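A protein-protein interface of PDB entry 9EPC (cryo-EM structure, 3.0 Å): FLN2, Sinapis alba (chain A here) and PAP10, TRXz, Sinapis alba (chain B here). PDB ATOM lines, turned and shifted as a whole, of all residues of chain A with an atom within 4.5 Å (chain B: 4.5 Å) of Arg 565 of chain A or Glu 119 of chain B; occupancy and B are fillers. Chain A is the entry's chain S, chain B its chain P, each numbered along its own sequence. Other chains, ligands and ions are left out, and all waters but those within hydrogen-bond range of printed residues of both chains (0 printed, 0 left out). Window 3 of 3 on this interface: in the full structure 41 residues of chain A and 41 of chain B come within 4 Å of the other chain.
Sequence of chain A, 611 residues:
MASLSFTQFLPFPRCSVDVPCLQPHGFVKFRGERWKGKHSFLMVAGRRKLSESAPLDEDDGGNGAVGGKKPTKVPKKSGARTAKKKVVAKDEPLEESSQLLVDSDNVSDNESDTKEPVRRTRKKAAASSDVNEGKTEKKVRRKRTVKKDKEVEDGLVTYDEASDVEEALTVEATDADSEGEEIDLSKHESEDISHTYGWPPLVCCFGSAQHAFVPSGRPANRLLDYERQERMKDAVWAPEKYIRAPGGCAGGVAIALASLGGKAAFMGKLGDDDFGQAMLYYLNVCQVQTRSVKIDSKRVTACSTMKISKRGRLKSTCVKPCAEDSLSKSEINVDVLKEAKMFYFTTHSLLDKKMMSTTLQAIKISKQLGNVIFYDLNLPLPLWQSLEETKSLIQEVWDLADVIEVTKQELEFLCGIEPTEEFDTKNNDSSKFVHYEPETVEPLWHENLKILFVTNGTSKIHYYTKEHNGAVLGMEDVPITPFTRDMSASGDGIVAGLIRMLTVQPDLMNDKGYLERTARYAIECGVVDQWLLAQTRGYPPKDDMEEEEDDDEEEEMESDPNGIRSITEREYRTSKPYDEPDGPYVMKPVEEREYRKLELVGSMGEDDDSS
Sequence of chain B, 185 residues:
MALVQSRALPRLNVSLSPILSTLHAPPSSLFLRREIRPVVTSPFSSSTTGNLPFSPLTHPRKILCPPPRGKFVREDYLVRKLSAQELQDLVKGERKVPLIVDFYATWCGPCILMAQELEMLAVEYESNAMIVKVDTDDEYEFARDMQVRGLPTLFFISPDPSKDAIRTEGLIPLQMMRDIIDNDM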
ATOM      1  N   PHE A 483       4.101  20.313   9.626  1.00  0.00           N
ATOM      2  CA  PHE A 483       3.645  18.935   9.509  1.00  0.00           C
ATOM      3  C   PHE A 483       3.351  18.530   8.073  1.00  0.00           C
ATOM      4  O   PHE A 483       3.302  17.332   7.783  1.00  0.00           O
ATOM      5  CB  PHE A 483       2.396  18.719  10.361  1.00  0.00           C
ATOM      6  CG  PHE A 483       2.638  18.848  11.836  1.00  0.00           C
ATOM      7  CD1 PHE A 483       3.909  18.706  12.358  1.00  0.00           C
ATOM      8  CD2 PHE A 483       1.591  19.107  12.699  1.00  0.00           C
ATOM      9  CE1 PHE A 483       4.130  18.825  13.711  1.00  0.00           C
ATOM     10  CE2 PHE A 483       1.808  19.225  14.053  1.00  0.00           C
ATOM     11  CZ  PHE A 483       3.078  19.085  14.560  1.00  0.00           C
ATOM     12  N   TYR A 539      -0.607  23.021  12.996  1.00  0.00           N
ATOM     13  CA  TYR A 539       0.748  23.504  13.192  1.00  0.00           C
ATOM     14  C   TYR A 539       1.306  23.003  14.517  1.00  0.00           C
ATOM     15  O   TYR A 539       0.554  22.802  15.474  1.00  0.00           O
ATOM     16  CB  TYR A 539       0.793  25.037  13.178  1.00  0.00           C
ATOM     17  CG  TYR A 539       0.385  25.668  11.869  1.00  0.00           C
ATOM     18  CD1 TYR A 539      -0.938  25.666  11.456  1.00  0.00           C
ATOM     19  CD2 TYR A 539       1.323  26.279  11.053  1.00  0.00           C
ATOM     20  CE1 TYR A 539      -1.313  26.243  10.263  1.00  0.00           C
ATOM     21  CE2 TYR A 539       0.957  26.859   9.860  1.00  0.00           C
ATOM     22  CZ  TYR A 539      -0.362  26.839   9.470  1.00  0.00           C
ATOM     23  OH  TYR A 539      -0.731  27.418   8.280  1.00  0.00           O
ATOM     24  N   PRO A 540       2.621  22.793  14.607  1.00  0.00           N
ATOM     25  CA  PRO A 540       3.217  22.470  15.897  1.00  0.00           C
ATOM     26  C   PRO A 540       3.096  23.651  16.847  1.00  0.00           C
ATOM     27  O   PRO A 540       3.066  24.812  16.410  1.00  0.00           O
ATOM     28  CB  PRO A 540       4.686  22.179  15.546  1.00  0.00           C
ATOM     29  CG  PRO A 540       4.919  22.924  14.292  1.00  0.00           C
ATOM     30  CD  PRO A 540       3.628  22.848  13.536  1.00  0.00           C
ATOM     31  N   PRO A 541       3.023  23.398  18.150  1.00  0.00           N
ATOM     32  CA  PRO A 541       2.825  24.498  19.098  1.00  0.00           C
ATOM     33  C   PRO A 541       4.023  25.431  19.140  1.00  0.00           C
ATOM     34  O   PRO A 541       5.159  25.041  18.865  1.00  0.00           O
ATOM     35  CB  PRO A 541       2.633  23.780  20.437  1.00  0.00           C
ATOM     36  CG  PRO A 541       3.348  22.493  20.265  1.00  0.00           C
ATOM     37  CD  PRO A 541       3.167  22.103  18.831  1.00  0.00           C
ATOM     38  N   GLY A 563       1.775  10.884  21.622  1.00  0.00           N
ATOM     39  CA  GLY A 563       2.067  12.270  21.927  1.00  0.00           C
ATOM     40  C   GLY A 563       2.256  13.119  20.692  1.00  0.00           C
ATOM     41  O   GLY A 563       3.300  13.065  20.035  1.00  0.00           O
ATOM     42  N   ILE A 564       1.241  13.920  20.377  1.00  0.00           N
ATOM     43  CA  ILE A 564       1.230  14.773  19.195  1.00  0.00           C
ATOM     44  C   ILE A 564       0.503  16.052  19.579  1.00  0.00           C
ATOM     45  O   ILE A 564      -0.715  16.038  19.788  1.00  0.00           O
ATOM     46  CB  ILE A 564       0.548  14.109  17.991  1.00  0.00           C
ATOM     47  CG1 ILE A 564       1.404  12.961  17.453  1.00  0.00           C
ATOM     48  CG2 ILE A 564       0.297  15.128  16.899  1.00  0.00           C
ATOM     49  CD1 ILE A 564       0.777  12.230  16.298  1.00  0.00           C
ATOM     50  N   ARG A 565       1.239  17.150  19.675  1.00  0.00           N
ATOM     51  CA  ARG A 565       0.673  18.440  20.032  1.00  0.00           C
ATOM     52  C   ARG A 565       0.584  19.305  18.785  1.00  0.00           C
ATOM     53  O   ARG A 565       1.584  19.498  18.087  1.00  0.00           O
ATOM     54  CB  ARG A 565       1.521  19.119  21.106  1.00  0.00           C
ATOM     55  CG  ARG A 565       1.516  18.372  22.430  1.00  0.00           C
ATOM     56  CD  ARG A 565       2.650  18.806  23.339  1.00  0.00           C
ATOM     57  NE  ARG A 565       3.955  18.551  22.743  1.00  0.00           N
ATOM     58  CZ  ARG A 565       4.842  19.491  22.450  1.00  0.00           C
ATOM     59  NH1 ARG A 565       4.613  20.765  22.722  1.00  0.00           N
ATOM     60  NH2 ARG A 565       5.992  19.143  21.880  1.00  0.00           N
ATOM     61  N   SER A 566      -0.615  19.804  18.498  1.00  0.00           N
ATOM     62  CA  SER A 566      -0.841  20.626  17.322  1.00  0.00           C
ATOM     63  C   SER A 566      -1.773  21.773  17.676  1.00  0.00           C
ATOM     64  O   SER A 566      -2.554  21.698  18.626  1.00  0.00           O
ATOM     65  CB  SER A 566      -1.432  19.815  16.165  1.00  0.00           C
ATOM     66  OG  SER A 566      -2.783  19.484  16.428  1.00  0.00           O
ATOM     67  N   ALA B 115       8.962  13.063  15.621  1.00  0.00           N
ATOM     68  CA  ALA B 115       9.775  13.551  16.729  1.00  0.00           C
ATOM     69  C   ALA B 115       8.945  13.717  17.995  1.00  0.00           C
ATOM     70  O   ALA B 115       9.390  13.346  19.087  1.00  0.00           O
ATOM     71  CB  ALA B 115      10.443  14.870  16.348  1.00  0.00           C
ATOM     72  N   GLN B 116       7.730  14.255  17.868  1.00  0.00           N
ATOM     73  CA  GLN B 116       6.910  14.518  19.048  1.00  0.00           C
ATOM     74  C   GLN B 116       6.597  13.236  19.804  1.00  0.00           C
ATOM     75  O   GLN B 116       6.565  13.229  21.039  1.00  0.00           O
ATOM     76  CB  GLN B 116       5.622  15.232  18.648  1.00  0.00           C
ATOM     77  CG  GLN B 116       5.835  16.652  18.173  1.00  0.00           C
ATOM     78  CD  GLN B 116       4.537  17.355  17.855  1.00  0.00           C
ATOM     79  OE1 GLN B 116       3.469  16.747  17.877  1.00  0.00           O
ATOM     80  NE2 GLN B 116       4.622  18.645  17.561  1.00  0.00           N
ATOM     81  N   GLU B 117       6.346  12.143  19.081  1.00  0.00           N
ATOM     82  CA  GLU B 117       6.165  10.856  19.743  1.00  0.00           C
ATOM     83  C   GLU B 117       7.438  10.428  20.458  1.00  0.00           C
ATOM     84  O   GLU B 117       7.395   9.934  21.589  1.00  0.00           O
ATOM     85  CB  GLU B 117       5.741   9.800  18.728  1.00  0.00           C
ATOM     86  CG  GLU B 117       4.414  10.078  18.067  1.00  0.00           C
ATOM     87  CD  GLU B 117       4.041   8.993  17.090  1.00  0.00           C
ATOM     88  OE1 GLU B 117       4.893   8.121  16.833  1.00  0.00           O
ATOM     89  OE2 GLU B 117       2.903   9.005  16.584  1.00  0.00           O
ATOM     90  N   LEU B 118       8.588  10.608  19.808  1.00  0.00           N
ATOM     91  CA  LEU B 118       9.853  10.280  20.446  1.00  0.00           C
ATOM     92  C   LEU B 118      10.193  11.237  21.577  1.00  0.00           C
ATOM     93  O   LEU B 118      10.930  10.857  22.491  1.00  0.00           O
ATOM     94  CB  LEU B 118      10.980  10.278  19.416  1.00  0.00           C
ATOM     95  CG  LEU B 118      10.872   9.228  18.313  1.00  0.00           C
ATOM     96  CD1 LEU B 118      12.115   9.249  17.446  1.00  0.00           C
ATOM     97  CD2 LEU B 118      10.656   7.851  18.909  1.00  0.00           C
ATOM     98  N   GLU B 119       9.678  12.469  21.534  1.00  0.00           N
ATOM     99  CA  GLU B 119       9.913  13.399  22.632  1.00  0.00           C
ATOM    100  C   GLU B 119       9.324  12.870  23.932  1.00  0.00           C
ATOM    101  O   GLU B 119       9.963  12.944  24.986  1.00  0.00           O
ATOM    102  CB  GLU B 119       9.324  14.770  22.302  1.00  0.00           C
ATOM    103  CG  GLU B 119      10.275  15.731  21.598  1.00  0.00           C
ATOM    104  CD  GLU B 119       9.620  17.046  21.230  1.00  0.00           C
ATOM    105  OE1 GLU B 119       8.381  17.151  21.348  1.00  0.00           O
ATOM    106  OE2 GLU B 119      10.346  17.981  20.830  1.00  0.00           O
ATOM    107  N   MET B 120       8.107  12.332  23.878  1.00  0.00           N
ATOM    108  CA  MET B 120       7.479  11.790  25.073  1.00  0.00           C
ATOM    109  C   MET B 120       7.793  10.318  25.295  1.00  0.00           C
ATOM    110  O   MET B 120       7.696   9.847  26.433  1.00  0.00           O
ATOM    111  CB  MET B 120       5.961  11.981  25.020  1.00  0.00           C
ATOM    112  CG  MET B 120       5.243  11.093  24.028  1.00  0.00           C
ATOM    113  SD  MET B 120       3.596  10.667  24.616  1.00  0.00           S
ATOM    114  CE  MET B 120       2.839  12.286  24.716  1.00  0.00           C
ATOM    115  N   LEU B 121       8.157   9.580  24.244  1.00  0.00           N
ATOM    116  CA  LEU B 121       8.629   8.216  24.445  1.00  0.00           C
ATOM    117  C   LEU B 121       9.919   8.206  25.251  1.00  0.00           C
ATOM    118  O   LEU B 121      10.108   7.354  26.127  1.00  0.00           O
ATOM    119  CB  LEU B 121       8.837   7.521  23.101  1.00  0.00           C
ATOM    120  CG  LEU B 121       9.258   6.056  23.186  1.00  0.00           C
ATOM    121  CD1 LEU B 121       8.141   5.220  23.778  1.00  0.00           C
ATOM    122  CD2 LEU B 121       9.659   5.530  21.822  1.00  0.00           C
ATOM    123  N   ALA B 122      10.818   9.149  24.967  1.00  0.00           N
ATOM    124  CA  ALA B 122      12.032   9.279  25.763  1.00  0.00           C
ATOM    125  C   ALA B 122      11.703   9.628  27.207  1.00  0.00           C
ATOM    126  O   ALA B 122      12.338   9.119  28.136  1.00  0.00           O
ATOM    127  CB  ALA B 122      12.951  10.334  25.152  1.00  0.00           C
ATOM    128  N   VAL B 123      10.713  10.498  27.414  1.00  0.00           N
ATOM    129  CA  VAL B 123      10.292  10.838  28.770  1.00  0.00           C
ATOM    130  C   VAL B 123       9.736   9.610  29.477  1.00  0.00           C
ATOM    131  O   VAL B 123      10.046   9.355  30.648  1.00  0.00           O
ATOM    132  CB  VAL B 123       9.267  11.985  28.737  1.00  0.00           C
ATOM    133  CG1 VAL B 123       8.664  12.197  30.113  1.00  0.00           C
ATOM    134  CG2 VAL B 123       9.921  13.259  28.238  1.00  0.00           C
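N of Glu 117 of chain B sits at hydrogen-bond distance from O of Gly 563 of chain A (3.3 Å). SD of Met 120 of chain B sits close to N of Gly 563 of chain A (3.5 Å). The guanidinium group of Arg 565 of chain A lies within salt-bridge range of the side-chain carboxylate of Glu 119 of chain B, at 3.2 Å. The side-chain amide oxygen of Gln 116 of chain B is in hydrogen-bond range of the backbone NH of Arg 565 of chain A (2.9 Å). The backbone carbonyl oxygen (O) of Gly 563 of chain A lies close to the backbone carbonyl oxygen (O) of Gln 116 of chain B (3.4 Å).
Among the printed residues, pairs that only touch across the chains: Phe 483 of chain A with Gln 116 of chain B (3.4 Å), Pro 541 of chain A with Gln 116 of chain B (3.96 Å), Ile 564 of chain A with Gln 116 of chain B (3.3 Å) and Ile 564 of chain A with Glu 117 of chain B (3.9 Å).
Of the printed residues of chain B, Phe 483 of chain A touches Gln 116 (3.4 Å). Tyr 539 of chain A touches none of the printed residues of chain B. Of the printed residues of chain B, Pro 541 of chain A touches Gln 116 (3.96 Å). Of the printed residues of chain B, Gly 563 of chain A touches Gln 116, Glu 117 and Met 120. Printed residues of chain B within 4 Å of Ile 564 of chain A: Gln 116 (3.3 Å) and Glu 117 (3.9 Å). Of chain B, only Gln 116 (2.9 Å) and Glu 119 (3.2 Å) come within 4 Å of Arg 565 of chain A. Of chain A, only Arg 565 (3.2 Å) comes within 4 Å of Glu 119 of chain B. The nearest printed residue of chain B that does not touch Arg 565 of chain A is Met 120 of chain B (6.6 Å). The nearest printed residue of chain A that does not touch Glu 119 of chain B is Gly 563 of chain A (6.6 Å).
Hydrophobic or aromatic side chains of chain B within 4 Å of the printed part of chain A: Met 120. Hydrophobic or aromatic side chains of chain A within 4 Å of the printed part of chain B: Phe 483, Pro 541 and Ile 564. Along chain A the printed residues that touch a printed residue of chain B span positions 483 to 565. Among the printed residues, Asp or Glu carboxylates within 4 Å of a Lys or Arg side-chain nitrogen of the other chain: Arg 565 of chain A with Glu 119 of chain B (3.2 Å).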
